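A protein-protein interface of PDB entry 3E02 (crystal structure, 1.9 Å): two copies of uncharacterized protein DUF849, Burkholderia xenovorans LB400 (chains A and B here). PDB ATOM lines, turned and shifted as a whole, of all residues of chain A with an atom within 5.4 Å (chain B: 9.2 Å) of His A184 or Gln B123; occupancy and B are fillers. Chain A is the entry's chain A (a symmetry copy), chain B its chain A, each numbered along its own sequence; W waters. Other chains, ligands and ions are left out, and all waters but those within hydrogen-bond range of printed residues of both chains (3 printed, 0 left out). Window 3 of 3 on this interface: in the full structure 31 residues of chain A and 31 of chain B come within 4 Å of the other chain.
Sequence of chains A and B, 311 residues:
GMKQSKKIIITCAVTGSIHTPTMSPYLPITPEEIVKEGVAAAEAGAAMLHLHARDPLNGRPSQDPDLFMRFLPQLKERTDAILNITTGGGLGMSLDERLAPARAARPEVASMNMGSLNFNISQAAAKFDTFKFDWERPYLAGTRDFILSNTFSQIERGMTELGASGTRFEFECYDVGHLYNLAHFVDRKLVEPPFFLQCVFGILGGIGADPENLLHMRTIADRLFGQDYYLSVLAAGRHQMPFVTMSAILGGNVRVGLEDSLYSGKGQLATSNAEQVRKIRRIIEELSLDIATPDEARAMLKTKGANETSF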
ATOM      1  N   PHE A 152     -15.438   5.308   3.746  1.00  0.00           N
ATOM      2  CA  PHE A 152     -14.169   4.607   3.515  1.00  0.00           C
ATOM      3  C   PHE A 152     -13.255   5.391   2.554  1.00  0.00           C
ATOM      4  O   PHE A 152     -12.061   5.483   2.791  1.00  0.00           O
ATOM      5  CB  PHE A 152     -14.401   3.159   3.067  1.00  0.00           C
ATOM      6  CG  PHE A 152     -14.805   2.263   4.194  1.00  0.00           C
ATOM      7  CD1 PHE A 152     -16.140   2.131   4.561  1.00  0.00           C
ATOM      8  CD2 PHE A 152     -13.843   1.580   4.922  1.00  0.00           C
ATOM      9  CE1 PHE A 152     -16.508   1.301   5.623  1.00  0.00           C
ATOM     10  CE2 PHE A 152     -14.195   0.755   5.981  1.00  0.00           C
ATOM     11  CZ  PHE A 152     -15.516   0.618   6.336  1.00  0.00           C
ATOM     12  N   LEU A 179     -14.120   0.100  15.000  1.00  0.00           N
ATOM     13  CA  LEU A 179     -12.964  -0.781  15.222  1.00  0.00           C
ATOM     14  C   LEU A 179     -12.737  -1.656  13.986  1.00  0.00           C
ATOM     15  O   LEU A 179     -11.606  -1.795  13.512  1.00  0.00           O
ATOM     16  CB  LEU A 179     -13.160  -1.652  16.471  1.00  0.00           C
ATOM     17  CG  LEU A 179     -13.360  -0.912  17.801  1.00  0.00           C
ATOM     18  CD1 LEU A 179     -13.735  -1.892  18.913  1.00  0.00           C
ATOM     19  CD2 LEU A 179     -12.104  -0.128  18.135  1.00  0.00           C
ATOM     20  N   TYR A 180     -13.827  -2.220  13.468  1.00  0.00           N
ATOM     21  CA  TYR A 180     -13.788  -3.027  12.260  1.00  0.00           C
ATOM     22  C   TYR A 180     -13.399  -2.196  11.036  1.00  0.00           C
ATOM     23  O   TYR A 180     -12.678  -2.691  10.160  1.00  0.00           O
ATOM     24  CB  TYR A 180     -15.113  -3.760  12.046  1.00  0.00           C
ATOM     25  CG  TYR A 180     -15.327  -4.826  13.088  1.00  0.00           C
ATOM     26  CD1 TYR A 180     -14.812  -6.105  12.918  1.00  0.00           C
ATOM     27  CD2 TYR A 180     -16.031  -4.549  14.271  1.00  0.00           C
ATOM     28  CE1 TYR A 180     -15.004  -7.105  13.909  1.00  0.00           C
ATOM     29  CE2 TYR A 180     -16.210  -5.522  15.258  1.00  0.00           C
ATOM     30  CZ  TYR A 180     -15.715  -6.797  15.065  1.00  0.00           C
ATOM     31  OH  TYR A 180     -15.920  -7.736  16.040  1.00  0.00           O
ATOM     32  N   ASN A 181     -13.877  -0.952  10.979  1.00  0.00           N
ATOM     33  CA  ASN A 181     -13.483   0.000   9.900  1.00  0.00           C
ATOM     34  C   ASN A 181     -11.968   0.221   9.940  1.00  0.00           C
ATOM     35  O   ASN A 181     -11.319   0.172   8.901  1.00  0.00           O
ATOM     36  CB  ASN A 181     -14.205   1.353  10.031  1.00  0.00           C
ATOM     37  CG  ASN A 181     -15.711   1.253   9.826  1.00  0.00           C
ATOM     38  OD1 ASN A 181     -16.239   0.192   9.469  1.00  0.00           O
ATOM     39  ND2 ASN A 181     -16.409   2.375  10.046  1.00  0.00           N
ATOM     40  N   LEU A 182     -11.411   0.442  11.135  1.00  0.00           N
ATOM     41  CA  LEU A 182      -9.951   0.598  11.285  1.00  0.00           C
ATOM     42  C   LEU A 182      -9.195  -0.663  10.870  1.00  0.00           C
ATOM     43  O   LEU A 182      -8.169  -0.572  10.167  1.00  0.00           O
ATOM     44  CB  LEU A 182      -9.569   0.987  12.720  1.00  0.00           C
ATOM     45  CG  LEU A 182      -8.076   1.257  12.965  1.00  0.00           C
ATOM     46  CD1 LEU A 182      -7.515   2.359  12.038  1.00  0.00           C
ATOM     47  CD2 LEU A 182      -7.921   1.631  14.399  1.00  0.00           C
ATOM     48  N   ALA A 183      -9.696  -1.829  11.292  1.00  0.00           N
ATOM     49  CA  ALA A 183      -9.091  -3.132  10.929  1.00  0.00           C
ATOM     50  C   ALA A 183      -8.957  -3.310   9.404  1.00  0.00           C
ATOM     51  O   ALA A 183      -7.947  -3.842   8.923  1.00  0.00           O
ATOM     52  CB  ALA A 183      -9.876  -4.290  11.557  1.00  0.00           C
ATOM     53  N   HIS A 184      -9.968  -2.860   8.661  1.00  0.00           N
ATOM     54  CA  HIS A 184      -9.947  -2.857   7.193  1.00  0.00           C
ATOM     55  C   HIS A 184      -8.687  -2.140   6.659  1.00  0.00           C
ATOM     56  O   HIS A 184      -7.978  -2.676   5.796  1.00  0.00           O
ATOM     57  CB  HIS A 184     -11.242  -2.216   6.639  1.00  0.00           C
ATOM     58  CG  HIS A 184     -11.219  -1.957   5.167  1.00  0.00           C
ATOM     59  ND1 HIS A 184     -11.442  -2.944   4.234  1.00  0.00           N
ATOM     60  CD2 HIS A 184     -10.981  -0.822   4.470  1.00  0.00           C
ATOM     61  CE1 HIS A 184     -11.359  -2.423   3.025  1.00  0.00           C
ATOM     62  NE2 HIS A 184     -11.081  -1.137   3.141  1.00  0.00           N
ATOM     63  N   PHE A 185      -8.410  -0.962   7.215  1.00  0.00           N
ATOM     64  CA  PHE A 185      -7.243  -0.144   6.825  1.00  0.00           C
ATOM     65  C   PHE A 185      -5.927  -0.704   7.347  1.00  0.00           C
ATOM     66  O   PHE A 185      -4.914  -0.684   6.627  1.00  0.00           O
ATOM     67  CB  PHE A 185      -7.451   1.312   7.238  1.00  0.00           C
ATOM     68  CG  PHE A 185      -8.519   1.981   6.447  1.00  0.00           C
ATOM     69  CD1 PHE A 185      -8.288   2.284   5.104  1.00  0.00           C
ATOM     70  CD2 PHE A 185      -9.759   2.263   6.996  1.00  0.00           C
ATOM     71  CE1 PHE A 185      -9.278   2.883   4.315  1.00  0.00           C
ATOM     72  CE2 PHE A 185     -10.760   2.877   6.225  1.00  0.00           C
ATOM     73  CZ  PHE A 185     -10.518   3.176   4.881  1.00  0.00           C
ATOM     74  N   VAL A 186      -5.945  -1.207   8.585  1.00  0.00           N
ATOM     75  CA  VAL A 186      -4.772  -1.852   9.181  1.00  0.00           C
ATOM     76  C   VAL A 186      -4.362  -3.061   8.325  1.00  0.00           C
ATOM     77  O   VAL A 186      -3.189  -3.177   7.971  1.00  0.00           O
ATOM     78  CB  VAL A 186      -4.991  -2.257  10.649  1.00  0.00           C
ATOM     79  CG1 VAL A 186      -3.843  -3.164  11.163  1.00  0.00           C
ATOM     80  CG2 VAL A 186      -5.148  -1.007  11.516  1.00  0.00           C
ATOM     81  N   ASP A 187      -5.326  -3.906   7.951  1.00  0.00           N
ATOM     82  CA  ASP A 187      -5.061  -5.067   7.071  1.00  0.00           C
ATOM     83  C   ASP A 187      -4.501  -4.676   5.698  1.00  0.00           C
ATOM     84  O   ASP A 187      -3.706  -5.428   5.124  1.00  0.00           O
ATOM     85  CB  ASP A 187      -6.307  -5.947   6.896  1.00  0.00           C
ATOM     86  CG  ASP A 187      -6.743  -6.627   8.187  1.00  0.00           C
ATOM     87  OD1 ASP A 187      -5.958  -6.678   9.171  1.00  0.00           O
ATOM     88  OD2 ASP A 187      -7.907  -7.086   8.230  1.00  0.00           O
ATOM     89  N   ARG A 188      -4.899  -3.511   5.188  1.00  0.00           N
ATOM     90  CA  ARG A 188      -4.372  -2.976   3.923  1.00  0.00           C
ATOM     91  C   ARG A 188      -3.075  -2.159   4.084  1.00  0.00           C
ATOM     92  O   ARG A 188      -2.556  -1.623   3.094  1.00  0.00           O
ATOM     93  CB  ARG A 188      -5.425  -2.115   3.239  1.00  0.00           C
ATOM     94  CG  ARG A 188      -6.638  -2.901   2.766  1.00  0.00           C
ATOM     95  CD  ARG A 188      -7.716  -1.955   2.339  1.00  0.00           C
ATOM     96  NE  ARG A 188      -7.245  -1.125   1.234  1.00  0.00           N
ATOM     97  CZ  ARG A 188      -7.782   0.021   0.823  1.00  0.00           C
ATOM     98  NH1 ARG A 188      -8.852   0.552   1.413  1.00  0.00           N
ATOM     99  NH2 ARG A 188      -7.217   0.652  -0.208  1.00  0.00           N
ATOM    100  N   MET B  23     -23.578 -12.352  -9.406  1.00  0.00           N
ATOM    101  CA  MET B  23     -23.166 -13.154  -8.249  1.00  0.00           C
ATOM    102  C   MET B  23     -23.839 -14.506  -8.105  1.00  0.00           C
ATOM    103  O   MET B  23     -23.285 -15.405  -7.473  1.00  0.00           O
ATOM    104  CB  MET B  23     -23.351 -12.346  -6.970  1.00  0.00           C
ATOM    105  CG  MET B  23     -22.644 -10.994  -7.032  1.00  0.00           C
ATOM    106  SD  MET B  23     -22.701 -10.094  -5.379  1.00  0.00           S
ATOM    107  CE  MET B  23     -21.761  -8.555  -5.988  1.00  0.00           C
ATOM    108  N   ASN B 118     -21.522   3.951   7.290  1.00  0.00           N
ATOM    109  CA  ASN B 118     -20.823   3.540   6.067  1.00  0.00           C
ATOM    110  C   ASN B 118     -21.383   2.150   5.714  1.00  0.00           C
ATOM    111  O   ASN B 118     -21.655   1.353   6.611  1.00  0.00           O
ATOM    112  CB  ASN B 118     -19.316   3.420   6.289  1.00  0.00           C
ATOM    113  CG  ASN B 118     -18.639   4.755   6.492  1.00  0.00           C
ATOM    114  OD1 ASN B 118     -19.214   5.808   6.204  1.00  0.00           O
ATOM    115  ND2 ASN B 118     -17.396   4.720   6.967  1.00  0.00           N
ATOM    116  N   PHE B 119     -21.625   1.899   4.433  1.00  0.00           N
ATOM    117  CA  PHE B 119     -22.216   0.622   3.992  1.00  0.00           C
ATOM    118  C   PHE B 119     -21.420   0.255   2.743  1.00  0.00           C
ATOM    119  O   PHE B 119     -21.812   0.591   1.632  1.00  0.00           O
ATOM    120  CB  PHE B 119     -23.721   0.801   3.739  1.00  0.00           C
ATOM    121  CG  PHE B 119     -24.501  -0.480   3.804  1.00  0.00           C
ATOM    122  CD1 PHE B 119     -24.237  -1.526   2.912  1.00  0.00           C
ATOM    123  CD2 PHE B 119     -25.515  -0.647   4.752  1.00  0.00           C
ATOM    124  CE1 PHE B 119     -24.954  -2.732   2.983  1.00  0.00           C
ATOM    125  CE2 PHE B 119     -26.242  -1.847   4.831  1.00  0.00           C
ATOM    126  CZ  PHE B 119     -25.964  -2.885   3.943  1.00  0.00           C
ATOM    127  N   ASN B 120     -20.297  -0.426   2.966  1.00  0.00           N
ATOM    128  CA  ASN B 120     -19.300  -0.728   1.952  1.00  0.00           C
ATOM    129  C   ASN B 120     -19.358  -2.184   1.474  1.00  0.00           C
ATOM    130  O   ASN B 120     -18.928  -3.097   2.183  1.00  0.00           O
ATOM    131  CB  ASN B 120     -17.908  -0.383   2.527  1.00  0.00           C
ATOM    132  CG  ASN B 120     -16.776  -0.455   1.490  1.00  0.00           C
ATOM    133  OD1 ASN B 120     -16.987  -0.822   0.327  1.00  0.00           O
ATOM    134  ND2 ASN B 120     -15.562  -0.095   1.921  1.00  0.00           N
ATOM    135  N   ILE B 121     -19.889  -2.386   0.267  1.00  0.00           N
ATOM    136  CA  ILE B 121     -19.959  -3.727  -0.364  1.00  0.00           C
ATOM    137  C   ILE B 121     -19.021  -3.824  -1.584  1.00  0.00           C
ATOM    138  O   ILE B 121     -19.129  -4.771  -2.382  1.00  0.00           O
ATOM    139  CB  ILE B 121     -21.427  -4.116  -0.720  1.00  0.00           C
ATOM    140  CG1 ILE B 121     -22.059  -3.135  -1.734  1.00  0.00           C
ATOM    141  CG2 ILE B 121     -22.250  -4.196   0.569  1.00  0.00           C
ATOM    142  CD1 ILE B 121     -23.440  -3.507  -2.152  1.00  0.00           C
ATOM    143  N   SER B 122     -18.089  -2.868  -1.704  1.00  0.00           N
ATOM    144  CA  SER B 122     -17.166  -2.781  -2.839  1.00  0.00           C
ATOM    145  C   SER B 122     -16.215  -3.964  -2.998  1.00  0.00           C
ATOM    146  O   SER B 122     -15.835  -4.284  -4.118  1.00  0.00           O
ATOM    147  CB  SER B 122     -16.346  -1.488  -2.754  1.00  0.00           C
ATOM    148  OG  SER B 122     -15.438  -1.519  -1.657  1.00  0.00           O
ATOM    149  N   GLN B 123     -15.827  -4.595  -1.887  1.00  0.00           N
ATOM    150  CA  GLN B 123     -14.931  -5.764  -1.915  1.00  0.00           C
ATOM    151  C   GLN B 123     -15.507  -6.951  -2.707  1.00  0.00           C
ATOM    152  O   GLN B 123     -14.749  -7.753  -3.232  1.00  0.00           O
ATOM    153  CB  GLN B 123     -14.571  -6.212  -0.489  1.00  0.00           C
ATOM    154  CG  GLN B 123     -13.699  -5.193   0.270  1.00  0.00           C
ATOM    155  CD  GLN B 123     -13.514  -5.546   1.747  1.00  0.00           C
ATOM    156  OE1 GLN B 123     -14.493  -5.820   2.475  1.00  0.00           O
ATOM    157  NE2 GLN B 123     -12.261  -5.518   2.207  1.00  0.00           N
ATOM    158  N   ALA B 124     -16.837  -7.058  -2.767  1.00  0.00           N
ATOM    159  CA  ALA B 124     -17.529  -8.095  -3.546  1.00  0.00           C
ATOM    160  C   ALA B 124     -17.138  -8.076  -5.031  1.00  0.00           C
ATOM    161  O   ALA B 124     -17.032  -9.137  -5.652  1.00  0.00           O
ATOM    162  CB  ALA B 124     -19.055  -7.960  -3.384  1.00  0.00           C
ATOM    163  N   ALA B 125     -16.875  -6.889  -5.574  1.00  0.00           N
ATOM    164  CA  ALA B 125     -16.498  -6.720  -6.986  1.00  0.00           C
ATOM    165  C   ALA B 125     -15.207  -7.442  -7.389  1.00  0.00           C
ATOM    166  O   ALA B 125     -15.095  -7.920  -8.525  1.00  0.00           O
ATOM    167  CB  ALA B 125     -16.407  -5.223  -7.347  1.00  0.00           C
ATOM    168  N   ALA B 126     -14.254  -7.543  -6.453  1.00  0.00           N
ATOM    169  CA  ALA B 126     -12.970  -8.224  -6.691  1.00  0.00           C
ATOM    170  C   ALA B 126     -13.112  -9.735  -6.932  1.00  0.00           C
ATOM    171  O   ALA B 126     -12.216 -10.350  -7.488  1.00  0.00           O
ATOM    172  CB  ALA B 126     -11.993  -7.962  -5.517  1.00  0.00           C
ATOM    173  N   LYS B 127     -14.229 -10.322  -6.506  1.00  0.00           N
ATOM    174  CA  LYS B 127     -14.508 -11.733  -6.729  1.00  0.00           C
ATOM    175  C   LYS B 127     -14.966 -12.069  -8.170  1.00  0.00           C
ATOM    176  O   LYS B 127     -15.018 -13.247  -8.519  1.00  0.00           O
ATOM    177  CB  LYS B 127     -15.557 -12.220  -5.743  1.00  0.00           C
ATOM    178  CG  LYS B 127     -15.135 -12.103  -4.289  1.00  0.00           C
ATOM    179  CD  LYS B 127     -16.276 -12.506  -3.398  1.00  0.00           C
ATOM    180  CE  LYS B 127     -15.853 -12.617  -1.953  1.00  0.00           C
ATOM    181  NZ  LYS B 127     -17.005 -13.103  -1.132  1.00  0.00           N
ATOM    182  N   PHE B 128     -15.274 -11.059  -8.992  1.00  0.00           N
ATOM    183  CA  PHE B 128     -15.796 -11.255 -10.358  1.00  0.00           C
ATOM    184  C   PHE B 128     -14.973 -10.453 -11.366  1.00  0.00           C
ATOM    185  O   PHE B 128     -14.841  -9.239 -11.228  1.00  0.00           O
ATOM    186  CB  PHE B 128     -17.282 -10.849 -10.393  1.00  0.00           C
ATOM    187  CG  PHE B 128     -18.089 -11.491  -9.306  1.00  0.00           C
ATOM    188  CD1 PHE B 128     -18.608 -12.776  -9.465  1.00  0.00           C
ATOM    189  CD2 PHE B 128     -18.251 -10.848  -8.076  1.00  0.00           C
ATOM    190  CE1 PHE B 128     -19.318 -13.387  -8.435  1.00  0.00           C
ATOM    191  CE2 PHE B 128     -18.952 -11.448  -7.026  1.00  0.00           C
ATOM    192  CZ  PHE B 128     -19.482 -12.731  -7.199  1.00  0.00           C
ATOM    193  N   PHE B 131     -18.901  -8.740 -15.441  1.00  0.00           N
ATOM    194  CA  PHE B 131     -20.249  -8.474 -14.943  1.00  0.00           C
ATOM    195  C   PHE B 131     -21.255  -8.524 -16.070  1.00  0.00           C
ATOM    196  O   PHE B 131     -20.970  -8.060 -17.179  1.00  0.00           O
ATOM    197  CB  PHE B 131     -20.301  -7.127 -14.223  1.00  0.00           C
ATOM    198  CG  PHE B 131     -19.727  -7.171 -12.846  1.00  0.00           C
ATOM    199  CD1 PHE B 131     -18.363  -6.960 -12.621  1.00  0.00           C
ATOM    200  CD2 PHE B 131     -20.546  -7.456 -11.765  1.00  0.00           C
ATOM    201  CE1 PHE B 131     -17.852  -7.025 -11.311  1.00  0.00           C
ATOM    202  CE2 PHE B 131     -20.038  -7.518 -10.472  1.00  0.00           C
ATOM    203  CZ  PHE B 131     -18.689  -7.306 -10.256  1.00  0.00           C
ATOM    204  N   ARG B 137     -20.888  -3.137 -11.501  1.00  0.00           N
ATOM    205  CA  ARG B 137     -19.578  -2.732 -10.974  1.00  0.00           C
ATOM    206  C   ARG B 137     -19.582  -1.299 -10.377  1.00  0.00           C
ATOM    207  O   ARG B 137     -19.078  -1.125  -9.266  1.00  0.00           O
ATOM    208  CB  ARG B 137     -18.443  -2.932 -11.978  1.00  0.00           C
ATOM    209  CG  ARG B 137     -17.076  -2.939 -11.304  1.00  0.00           C
ATOM    210  CD  ARG B 137     -15.898  -2.902 -12.281  1.00  0.00           C
ATOM    211  NE  ARG B 137     -15.598  -4.165 -12.964  1.00  0.00           N
ATOM    212  CZ  ARG B 137     -15.074  -5.256 -12.384  1.00  0.00           C
ATOM    213  NH1 ARG B 137     -14.796  -5.300 -11.078  1.00  0.00           N
ATOM    214  NH2 ARG B 137     -14.836  -6.344 -13.127  1.00  0.00           N
ATOM    215  N   TYR B 139     -22.097   0.368  -9.125  1.00  0.00           N
ATOM    216  CA  TYR B 139     -22.922   0.279  -7.915  1.00  0.00           C
ATOM    217  C   TYR B 139     -22.093  -0.192  -6.722  1.00  0.00           C
ATOM    218  O   TYR B 139     -22.063   0.463  -5.694  1.00  0.00           O
ATOM    219  CB  TYR B 139     -24.100  -0.670  -8.146  1.00  0.00           C
ATOM    220  CG  TYR B 139     -25.039  -0.863  -6.978  1.00  0.00           C
ATOM    221  CD1 TYR B 139     -25.944   0.140  -6.607  1.00  0.00           C
ATOM    222  CD2 TYR B 139     -25.065  -2.068  -6.269  1.00  0.00           C
ATOM    223  CE1 TYR B 139     -26.832  -0.054  -5.534  1.00  0.00           C
ATOM    224  CE2 TYR B 139     -25.945  -2.267  -5.209  1.00  0.00           C
ATOM    225  CZ  TYR B 139     -26.824  -1.261  -4.843  1.00  0.00           C
ATOM    226  OH  TYR B 139     -27.700  -1.469  -3.811  1.00  0.00           O
ATOM    227  N   LEU B 140     -21.394  -1.307  -6.890  1.00  0.00           N
ATOM    228  CA  LEU B 140     -20.549  -1.860  -5.829  1.00  0.00           C
ATOM    229  C   LEU B 140     -19.377  -0.928  -5.472  1.00  0.00           C
ATOM    230  O   LEU B 140     -19.147  -0.642  -4.290  1.00  0.00           O
ATOM    231  CB  LEU B 140     -20.031  -3.254  -6.224  1.00  0.00           C
ATOM    232  CG  LEU B 140     -21.090  -4.339  -6.470  1.00  0.00           C
ATOM    233  CD1 LEU B 140     -20.448  -5.577  -7.124  1.00  0.00           C
ATOM    234  CD2 LEU B 140     -21.869  -4.726  -5.218  1.00  0.00           C
ATOM    235  N   ALA B 141     -18.669  -0.448  -6.494  1.00  0.00           N
ATOM    236  CA  ALA B 141     -17.515   0.465  -6.322  1.00  0.00           C
ATOM    237  C   ALA B 141     -17.906   1.774  -5.629  1.00  0.00           C
ATOM    238  O   ALA B 141     -17.196   2.247  -4.743  1.00  0.00           O
ATOM    239  CB  ALA B 141     -16.841   0.738  -7.667  1.00  0.00           C
ATOM    240  N   GLY B 142     -19.064   2.313  -5.997  1.00  0.00           N
ATOM    241  CA  GLY B 142     -19.601   3.532  -5.411  1.00  0.00           C
ATOM    242  C   GLY B 142     -19.897   3.453  -3.920  1.00  0.00           C
ATOM    243  O   GLY B 142     -20.003   4.497  -3.267  1.00  0.00           O
ATOM    244  N   THR B 143     -20.001   2.237  -3.362  1.00  0.00           N
ATOM    245  CA  THR B 143     -20.259   2.069  -1.933  1.00  0.00           C
ATOM    246  C   THR B 143     -19.061   2.405  -1.035  1.00  0.00           C
ATOM    247  O   THR B 143     -19.255   2.561   0.178  1.00  0.00           O
ATOM    248  CB  THR B 143     -20.916   0.737  -1.573  1.00  0.00           C
ATOM    249  OG1 THR B 143     -20.010  -0.352  -1.775  1.00  0.00           O
ATOM    250  CG2 THR B 143     -22.232   0.553  -2.364  1.00  0.00           C
ATOM    251  N   ARG B 144     -17.850   2.533  -1.605  1.00  0.00           N
ATOM    252  CA  ARG B 144     -16.672   2.954  -0.836  1.00  0.00           C
ATOM    253  C   ARG B 144     -16.891   4.355  -0.266  1.00  0.00           C
ATOM    254  O   ARG B 144     -16.378   4.671   0.795  1.00  0.00           O
ATOM    255  CB  ARG B 144     -15.398   2.963  -1.691  1.00  0.00           C
ATOM    256  CG  ARG B 144     -14.960   1.622  -2.220  1.00  0.00           C
ATOM    257  CD  ARG B 144     -13.772   1.757  -3.159  1.00  0.00           C
ATOM    258  NE  ARG B 144     -14.154   2.279  -4.478  1.00  0.00           N
ATOM    259  CZ  ARG B 144     -13.311   2.781  -5.382  1.00  0.00           C
ATOM    260  NH1 ARG B 144     -11.989   2.820  -5.173  1.00  0.00           N
ATOM    261  NH2 ARG B 144     -13.803   3.242  -6.535  1.00  0.00           N
ATOM    262  N   GLY B 202     -21.838  -8.314  10.177  1.00  0.00           N
ATOM    263  CA  GLY B 202     -20.972  -8.601   9.039  1.00  0.00           C
ATOM    264  C   GLY B 202     -20.917  -7.615   7.897  1.00  0.00           C
ATOM    265  O   GLY B 202     -20.233  -7.889   6.923  1.00  0.00           O
ATOM    266  N   ILE B 203     -21.603  -6.477   7.996  1.00  0.00           N
ATOM    267  CA  ILE B 203     -21.520  -5.449   6.955  1.00  0.00           C
ATOM    268  C   ILE B 203     -20.287  -4.595   7.258  1.00  0.00           C
ATOM    269  O   ILE B 203     -20.089  -4.194   8.405  1.00  0.00           O
ATOM    270  CB  ILE B 203     -22.772  -4.542   6.914  1.00  0.00           C
ATOM    271  CG1 ILE B 203     -24.042  -5.363   6.622  1.00  0.00           C
ATOM    272  CG2 ILE B 203     -22.604  -3.395   5.889  1.00  0.00           C
ATOM    273  CD1 ILE B 203     -24.076  -6.014   5.245  1.00  0.00           C
ATOM    274  N   LEU B 204     -19.475  -4.311   6.232  1.00  0.00           N
ATOM    275  CA  LEU B 204     -18.306  -3.422   6.378  1.00  0.00           C
ATOM    276  C   LEU B 204     -18.855  -1.988   6.500  1.00  0.00           C
ATOM    277  O   LEU B 204     -19.408  -1.426   5.543  1.00  0.00           O
ATOM    278  CB  LEU B 204     -17.314  -3.565   5.217  1.00  0.00           C
ATOM    279  CG  LEU B 204     -16.023  -2.735   5.274  1.00  0.00           C
ATOM    280  CD1 LEU B 204     -15.284  -2.920   6.616  1.00  0.00           C
ATOM    281  CD2 LEU B 204     -15.093  -3.010   4.056  1.00  0.00           C
ATOM    282  N   GLY B 205     -18.672  -1.415   7.687  1.00  0.00           N
ATOM    283  CA  GLY B 205     -19.280  -0.159   8.098  1.00  0.00           C
ATOM    284  C   GLY B 205     -20.164  -0.391   9.325  1.00  0.00           C
ATOM    285  O   GLY B 205     -20.434   0.548  10.058  1.00  0.00           O
HETATM  286  O   HOH W   1     -18.447   3.992   2.875  1.00  0.00           O
HETATM  287  O   HOH W   2     -17.242  -2.336   9.923  1.00  0.00           O
HETATM  288  O   HOH W   3     -12.842   0.121   0.992  1.00  0.00           O
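Leu A182 touches none of the printed residues of chain B.
His A184 touches just these residues of chain B: Gln B123 and Leu B204.
No residue of chain B comes within 4 Å of Phe A185.
Of the printed residues of chain A, Asn B118 touches Phe A152 and Asn A181.
Of chain A, only His A184 (3.3 Å) comes within 4 Å of Gln B123.
Printed residues of chain A within 4 Å of Arg B144: Phe A152 (3.2 Å).
A ring nitrogen (ND1) of His A184 lies close to the side-chain amide nitrogen (NE2) of Gln B123 (3.4 Å).
The backbone carbonyl oxygen (O) of Arg B144 lies within hydrogen-bond range of the backbone NH (N) of Phe A152, at 3.2 Å.
N of Gly B205 lies close to OD1 of Asn A181 (3.4 Å).
Along chain A the printed residues that touch a printed residue of chain B span positions 152 to 184.
Printed residues of chain B that touch a printed residue of chain A: Asn B118, Asn B120, Gln B123, Arg B144, Leu B204 and Gly B205.
Hydrophobic or aromatic side chains of chain B within 4 Å of the printed part of chain A: Leu B204.
Among the printed residues, no Asp or Glu carboxylate lies within 4 Å of a Lys or Arg side-chain nitrogen of the other chain.
Phe A152 touches Asn B118 (CE1 to CB, 3.6 Å).
Asn B120 touches Phe A152 (ND2 to CG, 3.4 Å).
Phe A152 touches Leu B204 (CZ to CG, 3.6 Å).
Phe A152 touches Gly B205 (CZ to N, 3.99 Å).
Asn B118 touches Asn A181.
His A184 touches Leu B204 (ND1 to CD2, 3.7 Å).
No position is printed for both chains.
Of the 9 pairs that touch across the chains among the printed residues, none has its exchanged pair printed and touching as well.
Water W2 lies within hydrogen-bond range of OD1 of Asn A181 (2.8 Å) and N of Gly B205 (2.8 Å).
Water W3 bridges the side-chain amide nitrogen of Asn B120 and a ring nitrogen (NE2) of His A184.
Water W1 lies within hydrogen-bond range of the backbone carbonyl oxygen (O) of Arg B144, the backbone carbonyl oxygen (O) of Thr B143 and the backbone NH (N) of Phe A152.
The side-chain amide oxygen of Asn B120 lies within hydrogen-bond range of the side-chain hydroxyl of Ser B122 (2.6 Å).
N of Asn B120 lies within hydrogen-bond range of O of Leu B204.
O of Ala B141 lies within hydrogen-bond range of NE of Arg B144 (3.1 Å).
A ring nitrogen (NE2) of His A184 lies within hydrogen-bond range of the guanidinium group (NH1) of Arg A188 (3.3 Å).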
